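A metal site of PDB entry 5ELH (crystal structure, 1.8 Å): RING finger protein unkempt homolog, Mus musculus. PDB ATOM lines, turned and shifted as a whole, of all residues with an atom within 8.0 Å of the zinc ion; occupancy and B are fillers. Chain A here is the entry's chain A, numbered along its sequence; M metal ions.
The backbone NH of His 36 lies within hydrogen-bond range of the side-chain amide oxygen of Gln 40 (2.9 Å).
The backbone NH of Cys 32 lies within hydrogen-bond range of the backbone carbonyl oxygen of Gln 26, 3.3 Å away.
The backbone NH of Leu 18 sits close to the side-chain sulfur of Cys 16, at 3.5 Å.
N of Cys 24 sits at hydrogen-bond distance from O of Leu 18 (3.4 Å).
The side-chain sulfur of Cys 32 lies close to the backbone NH of His 34.
The backbone NH (N) of Cys 16 is in hydrogen-bond range of the backbone carbonyl oxygen (O) of Trp 35.
The backbone NH of Phe 19 lies close to the side-chain sulfur of Cys 16 (3.3 Å).
The side-chain sulfur of Cys 24 sits close to the backbone NH of Gln 26, at 3.4 Å.
The zinc ion is bound by a ring nitrogen (NE2) of His 36 (2.0 Å), the side-chain sulfur (SG) of Cys 16 (2.3 Å), the side-chain sulfur (SG) of Cys 24 (2.3 Å) and the side-chain sulfur (SG) of Cys 32 (2.4 Å).
Of the 21 residues printed, 4 come within 4 Å of the zinc ion.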
ATOM      1  N   ARG A  12      29.069 -12.297 -13.028  1.00  0.00           N
ATOM      2  CA  ARG A  12      29.249 -13.081 -14.251  1.00  0.00           C
ATOM      3  C   ARG A  12      30.404 -12.604 -15.108  1.00  0.00           C
ATOM      4  O   ARG A  12      30.388 -12.774 -16.329  1.00  0.00           O
ATOM      5  CB  ARG A  12      27.968 -13.071 -15.072  1.00  0.00           C
ATOM      6  CG  ARG A  12      26.774 -13.652 -14.344  1.00  0.00           C
ATOM      7  CD  ARG A  12      26.713 -15.148 -14.459  1.00  0.00           C
ATOM      8  NE  ARG A  12      25.520 -15.661 -13.797  1.00  0.00           N
ATOM      9  CZ  ARG A  12      24.284 -15.551 -14.282  1.00  0.00           C
ATOM     10  NH1 ARG A  12      24.057 -14.935 -15.447  1.00  0.00           N
ATOM     11  NH2 ARG A  12      23.275 -16.047 -13.603  1.00  0.00           N
ATOM     12  N   GLU A  14      33.724 -13.480 -14.268  1.00  0.00           N
ATOM     13  CA  GLU A  14      34.796 -14.474 -14.148  1.00  0.00           C
ATOM     14  C   GLU A  14      34.233 -15.884 -14.201  1.00  0.00           C
ATOM     15  O   GLU A  14      33.079 -16.112 -13.825  1.00  0.00           O
ATOM     16  CB  GLU A  14      35.560 -14.288 -12.836  1.00  0.00           C
ATOM     17  CG  GLU A  14      36.237 -12.932 -12.668  1.00  0.00           C
ATOM     18  CD  GLU A  14      37.426 -12.745 -13.576  1.00  0.00           C
ATOM     19  OE1 GLU A  14      38.021 -13.767 -14.002  1.00  0.00           O
ATOM     20  OE2 GLU A  14      37.764 -11.581 -13.873  1.00  0.00           O
ATOM     21  N   GLN A  15      35.067 -16.828 -14.628  1.00  0.00           N
ATOM     22  CA  GLN A  15      34.634 -18.206 -14.738  1.00  0.00           C
ATOM     23  C   GLN A  15      34.527 -18.867 -13.376  1.00  0.00           C
ATOM     24  O   GLN A  15      35.365 -18.650 -12.494  1.00  0.00           O
ATOM     25  CB  GLN A  15      35.616 -19.016 -15.595  1.00  0.00           C
ATOM     26  CG  GLN A  15      35.108 -20.400 -15.921  1.00  0.00           C
ATOM     27  CD  GLN A  15      36.091 -21.210 -16.749  1.00  0.00           C
ATOM     28  OE1 GLN A  15      37.303 -21.039 -16.659  1.00  0.00           O
ATOM     29  NE2 GLN A  15      35.554 -22.107 -17.567  1.00  0.00           N
ATOM     30  N   CYS A  16      33.499 -19.687 -13.212  1.00  0.00           N
ATOM     31  CA  CYS A  16      33.302 -20.434 -11.970  1.00  0.00           C
ATOM     32  C   CYS A  16      34.328 -21.570 -11.865  1.00  0.00           C
ATOM     33  O   CYS A  16      34.309 -22.501 -12.676  1.00  0.00           O
ATOM     34  CB  CYS A  16      31.883 -21.029 -11.953  1.00  0.00           C
ATOM     35  SG  CYS A  16      31.473 -22.008 -10.473  1.00  0.00           S
ATOM     36  N   PRO A  17      35.220 -21.508 -10.854  1.00  0.00           N
ATOM     37  CA  PRO A  17      36.205 -22.594 -10.691  1.00  0.00           C
ATOM     38  C   PRO A  17      35.583 -23.924 -10.261  1.00  0.00           C
ATOM     39  O   PRO A  17      36.200 -24.980 -10.439  1.00  0.00           O
ATOM     40  CB  PRO A  17      37.137 -22.058  -9.603  1.00  0.00           C
ATOM     41  CG  PRO A  17      36.308 -21.085  -8.837  1.00  0.00           C
ATOM     42  CD  PRO A  17      35.395 -20.448  -9.850  1.00  0.00           C
ATOM     43  N   LEU A  18      34.375 -23.889  -9.690  1.00  0.00           N
ATOM     44  CA  LEU A  18      33.706 -25.111  -9.274  1.00  0.00           C
ATOM     45  C   LEU A  18      33.049 -25.811 -10.466  1.00  0.00           C
ATOM     46  O   LEU A  18      33.060 -27.034 -10.556  1.00  0.00           O
ATOM     47  CB  LEU A  18      32.653 -24.829  -8.201  1.00  0.00           C
ATOM     48  CG  LEU A  18      33.133 -24.430  -6.793  1.00  0.00           C
ATOM     49  CD1 LEU A  18      31.930 -24.347  -5.870  1.00  0.00           C
ATOM     50  CD2 LEU A  18      34.165 -25.395  -6.239  1.00  0.00           C
ATOM     51  N   PHE A  19      32.463 -25.030 -11.373  1.00  0.00           N
ATOM     52  CA  PHE A  19      31.708 -25.601 -12.478  1.00  0.00           C
ATOM     53  C   PHE A  19      32.589 -26.455 -13.385  1.00  0.00           C
ATOM     54  O   PHE A  19      32.176 -27.520 -13.865  1.00  0.00           O
ATOM     55  CB  PHE A  19      31.032 -24.511 -13.317  1.00  0.00           C
ATOM     56  CG  PHE A  19      30.340 -25.053 -14.540  1.00  0.00           C
ATOM     57  CD1 PHE A  19      29.134 -25.729 -14.426  1.00  0.00           C
ATOM     58  CD2 PHE A  19      30.930 -24.934 -15.795  1.00  0.00           C
ATOM     59  CE1 PHE A  19      28.511 -26.245 -15.546  1.00  0.00           C
ATOM     60  CE2 PHE A  19      30.307 -25.440 -16.915  1.00  0.00           C
ATOM     61  CZ  PHE A  19      29.102 -26.106 -16.788  1.00  0.00           C
ATOM     62  N   VAL A  20      33.809 -25.991 -13.607  1.00  0.00           N
ATOM     63  CA  VAL A  20      34.737 -26.693 -14.485  1.00  0.00           C
ATOM     64  C   VAL A  20      35.029 -28.082 -13.949  1.00  0.00           C
ATOM     65  O   VAL A  20      35.495 -28.956 -14.690  1.00  0.00           O
ATOM     66  CB  VAL A  20      36.056 -25.905 -14.658  1.00  0.00           C
ATOM     67  CG1 VAL A  20      35.800 -24.504 -15.175  1.00  0.00           C
ATOM     68  CG2 VAL A  20      36.795 -25.800 -13.342  1.00  0.00           C
ATOM     69  N   LYS A  23      31.511 -29.407  -9.791  1.00  0.00           N
ATOM     70  CA  LYS A  23      31.356 -29.267  -8.347  1.00  0.00           C
ATOM     71  C   LYS A  23      30.489 -28.065  -7.989  1.00  0.00           C
ATOM     72  O   LYS A  23      30.245 -27.815  -6.812  1.00  0.00           O
ATOM     73  CB  LYS A  23      32.729 -29.108  -7.671  1.00  0.00           C
ATOM     74  CG  LYS A  23      33.601 -30.341  -7.689  1.00  0.00           C
ATOM     75  CD  LYS A  23      34.996 -30.004  -7.168  1.00  0.00           C
ATOM     76  CE  LYS A  23      35.901 -31.225  -7.103  1.00  0.00           C
ATOM     77  NZ  LYS A  23      37.288 -30.861  -6.695  1.00  0.00           N
ATOM     78  N   CYS A  24      30.041 -27.313  -8.989  1.00  0.00           N
ATOM     79  CA  CYS A  24      29.144 -26.194  -8.711  1.00  0.00           C
ATOM     80  C   CYS A  24      27.711 -26.695  -8.504  1.00  0.00           C
ATOM     81  O   CYS A  24      27.158 -27.373  -9.362  1.00  0.00           O
ATOM     82  CB  CYS A  24      29.177 -25.138  -9.803  1.00  0.00           C
ATOM     83  SG  CYS A  24      28.222 -23.656  -9.361  1.00  0.00           S
ATOM     84  N   THR A  25      27.144 -26.355  -7.347  1.00  0.00           N
ATOM     85  CA  THR A  25      25.788 -26.750  -6.990  1.00  0.00           C
ATOM     86  C   THR A  25      24.768 -25.722  -7.426  1.00  0.00           C
ATOM     87  O   THR A  25      23.577 -25.873  -7.135  1.00  0.00           O
ATOM     88  CB  THR A  25      25.638 -26.878  -5.463  1.00  0.00           C
ATOM     89  OG1 THR A  25      25.769 -25.589  -4.858  1.00  0.00           O
ATOM     90  CG2 THR A  25      26.691 -27.813  -4.903  1.00  0.00           C
ATOM     91  N   GLN A  26      25.236 -24.662  -8.089  1.00  0.00           N
ATOM     92  CA  GLN A  26      24.378 -23.547  -8.487  1.00  0.00           C
ATOM     93  C   GLN A  26      24.246 -23.447  -9.998  1.00  0.00           C
ATOM     94  O   GLN A  26      24.237 -22.350 -10.564  1.00  0.00           O
ATOM     95  CB  GLN A  26      24.931 -22.235  -7.921  1.00  0.00           C
ATOM     96  CG  GLN A  26      24.859 -22.132  -6.404  1.00  0.00           C
ATOM     97  CD  GLN A  26      25.459 -20.850  -5.889  1.00  0.00           C
ATOM     98  OE1 GLN A  26      26.393 -20.304  -6.488  1.00  0.00           O
ATOM     99  NE2 GLN A  26      24.934 -20.349  -4.774  1.00  0.00           N
ATOM    100  N   HIS A  27      24.151 -24.607 -10.650  1.00  0.00           N
ATOM    101  CA  HIS A  27      23.888 -24.699 -12.078  1.00  0.00           C
ATOM    102  C   HIS A  27      22.552 -25.406 -12.268  1.00  0.00           C
ATOM    103  O   HIS A  27      22.438 -26.582 -11.920  1.00  0.00           O
ATOM    104  CB  HIS A  27      24.986 -25.511 -12.765  1.00  0.00           C
ATOM    105  CG  HIS A  27      24.732 -25.774 -14.224  1.00  0.00           C
ATOM    106  ND1 HIS A  27      25.045 -24.866 -15.215  1.00  0.00           N
ATOM    107  CD2 HIS A  27      24.175 -26.827 -14.860  1.00  0.00           C
ATOM    108  CE1 HIS A  27      24.709 -25.355 -16.387  1.00  0.00           C
ATOM    109  NE2 HIS A  27      24.175 -26.549 -16.199  1.00  0.00           N
ATOM    110  N   TYR A  30      20.361 -22.124 -12.291  1.00  0.00           N
ATOM    111  CA  TYR A  30      21.613 -21.407 -12.444  1.00  0.00           C
ATOM    112  C   TYR A  30      21.607 -20.126 -11.612  1.00  0.00           C
ATOM    113  O   TYR A  30      21.250 -19.069 -12.100  1.00  0.00           O
ATOM    114  CB  TYR A  30      21.837 -21.095 -13.931  1.00  0.00           C
ATOM    115  CG  TYR A  30      23.114 -20.341 -14.236  1.00  0.00           C
ATOM    116  CD1 TYR A  30      24.328 -20.719 -13.664  1.00  0.00           C
ATOM    117  CD2 TYR A  30      23.109 -19.271 -15.120  1.00  0.00           C
ATOM    118  CE1 TYR A  30      25.495 -20.039 -13.960  1.00  0.00           C
ATOM    119  CE2 TYR A  30      24.269 -18.581 -15.409  1.00  0.00           C
ATOM    120  CZ  TYR A  30      25.454 -18.960 -14.836  1.00  0.00           C
ATOM    121  OH  TYR A  30      26.599 -18.260 -15.138  1.00  0.00           O
ATOM    122  N   THR A  31      21.996 -20.244 -10.342  1.00  0.00           N
ATOM    123  CA  THR A  31      22.041 -19.090  -9.438  1.00  0.00           C
ATOM    124  C   THR A  31      23.466 -18.629  -9.184  1.00  0.00           C
ATOM    125  O   THR A  31      23.715 -17.849  -8.261  1.00  0.00           O
ATOM    126  CB  THR A  31      21.443 -19.427  -8.071  1.00  0.00           C
ATOM    127  OG1 THR A  31      22.275 -20.396  -7.413  1.00  0.00           O
ATOM    128  CG2 THR A  31      20.027 -19.966  -8.211  1.00  0.00           C
ATOM    129  N   CYS A  32      24.413 -19.118  -9.976  1.00  0.00           N
ATOM    130  CA  CYS A  32      25.810 -18.837  -9.694  1.00  0.00           C
ATOM    131  C   CYS A  32      26.158 -17.403 -10.034  1.00  0.00           C
ATOM    132  O   CYS A  32      25.625 -16.811 -10.975  1.00  0.00           O
ATOM    133  CB  CYS A  32      26.752 -19.785 -10.439  1.00  0.00           C
ATOM    134  SG  CYS A  32      28.466 -19.716  -9.808  1.00  0.00           S
ATOM    135  N   PHE A  33      27.065 -16.845  -9.249  1.00  0.00           N
ATOM    136  CA  PHE A  33      27.529 -15.484  -9.445  1.00  0.00           C
ATOM    137  C   PHE A  33      28.538 -15.399 -10.595  1.00  0.00           C
ATOM    138  O   PHE A  33      28.800 -14.323 -11.134  1.00  0.00           O
ATOM    139  CB  PHE A  33      28.177 -14.992  -8.155  1.00  0.00           C
ATOM    140  CG  PHE A  33      28.362 -13.524  -8.104  1.00  0.00           C
ATOM    141  CD1 PHE A  33      27.301 -12.699  -7.746  1.00  0.00           C
ATOM    142  CD2 PHE A  33      29.573 -12.943  -8.428  1.00  0.00           C
ATOM    143  CE1 PHE A  33      27.461 -11.332  -7.705  1.00  0.00           C
ATOM    144  CE2 PHE A  33      29.740 -11.585  -8.380  1.00  0.00           C
ATOM    145  CZ  PHE A  33      28.687 -10.780  -8.029  1.00  0.00           C
ATOM    146  N   HIS A  34      29.089 -16.541 -10.980  1.00  0.00           N
ATOM    147  CA  HIS A  34      30.145 -16.602 -11.981  1.00  0.00           C
ATOM    148  C   HIS A  34      29.630 -17.229 -13.261  1.00  0.00           C
ATOM    149  O   HIS A  34      28.588 -17.882 -13.241  1.00  0.00           O
ATOM    150  CB  HIS A  34      31.301 -17.412 -11.409  1.00  0.00           C
ATOM    151  CG  HIS A  34      31.800 -16.895 -10.105  1.00  0.00           C
ATOM    152  ND1 HIS A  34      32.400 -15.652  -9.979  1.00  0.00           N
ATOM    153  CD2 HIS A  34      31.760 -17.417  -8.857  1.00  0.00           C
ATOM    154  CE1 HIS A  34      32.722 -15.452  -8.713  1.00  0.00           C
ATOM    155  NE2 HIS A  34      32.341 -16.508  -8.013  1.00  0.00           N
ATOM    156  N   TRP A  35      30.311 -17.034 -14.381  1.00  0.00           N
ATOM    157  CA  TRP A  35      29.854 -17.648 -15.622  1.00  0.00           C
ATOM    158  C   TRP A  35      30.312 -19.096 -15.703  1.00  0.00           C
ATOM    159  O   TRP A  35      31.372 -19.471 -15.201  1.00  0.00           O
ATOM    160  CB  TRP A  35      30.225 -16.845 -16.882  1.00  0.00           C
ATOM    161  CG  TRP A  35      31.674 -16.647 -17.210  1.00  0.00           C
ATOM    162  CD1 TRP A  35      32.428 -15.556 -16.962  1.00  0.00           C
ATOM    163  CD2 TRP A  35      32.519 -17.568 -17.922  1.00  0.00           C
ATOM    164  NE1 TRP A  35      33.702 -15.728 -17.448  1.00  0.00           N
ATOM    165  CE2 TRP A  35      33.776 -16.960 -18.044  1.00  0.00           C
ATOM    166  CE3 TRP A  35      32.329 -18.847 -18.445  1.00  0.00           C
ATOM    167  CZ2 TRP A  35      34.856 -17.581 -18.677  1.00  0.00           C
ATOM    168  CZ3 TRP A  35      33.403 -19.478 -19.071  1.00  0.00           C
ATOM    169  CH2 TRP A  35      34.646 -18.831 -19.179  1.00  0.00           C
ATOM    170  N   HIS A  36      29.464 -19.909 -16.328  1.00  0.00           N
ATOM    171  CA  HIS A  36      29.751 -21.325 -16.521  1.00  0.00           C
ATOM    172  C   HIS A  36      30.099 -21.569 -17.994  1.00  0.00           C
ATOM    173  O   HIS A  36      31.038 -22.298 -18.312  1.00  0.00           O
ATOM    174  CB  HIS A  36      28.556 -22.173 -16.077  1.00  0.00           C
ATOM    175  CG  HIS A  36      28.359 -22.234 -14.591  1.00  0.00           C
ATOM    176  ND1 HIS A  36      27.389 -23.022 -14.013  1.00  0.00           N
ATOM    177  CD2 HIS A  36      28.994 -21.610 -13.580  1.00  0.00           C
ATOM    178  CE1 HIS A  36      27.439 -22.879 -12.695  1.00  0.00           C
ATOM    179  NE2 HIS A  36      28.409 -22.041 -12.403  1.00  0.00           N
ATOM    180  N   GLN A  40      27.745 -16.829 -21.318  1.00  0.00           N
ATOM    181  CA  GLN A  40      27.156 -16.199 -20.125  1.00  0.00           C
ATOM    182  C   GLN A  40      28.011 -15.068 -19.572  1.00  0.00           C
ATOM    183  O   GLN A  40      27.563 -14.301 -18.708  1.00  0.00           O
ATOM    184  CB  GLN A  40      26.938 -17.231 -19.038  1.00  0.00           C
ATOM    185  CG  GLN A  40      26.008 -18.340 -19.417  1.00  0.00           C
ATOM    186  CD  GLN A  40      26.015 -19.467 -18.411  1.00  0.00           C
ATOM    187  OE1 GLN A  40      27.077 -19.851 -17.895  1.00  0.00           O
ATOM    188  NE2 GLN A  40      24.844 -20.008 -18.118  1.00  0.00           N
HETATM  189 ZN    ZN M   1      29.177 -21.852 -10.524  1.00  0.00          ZN
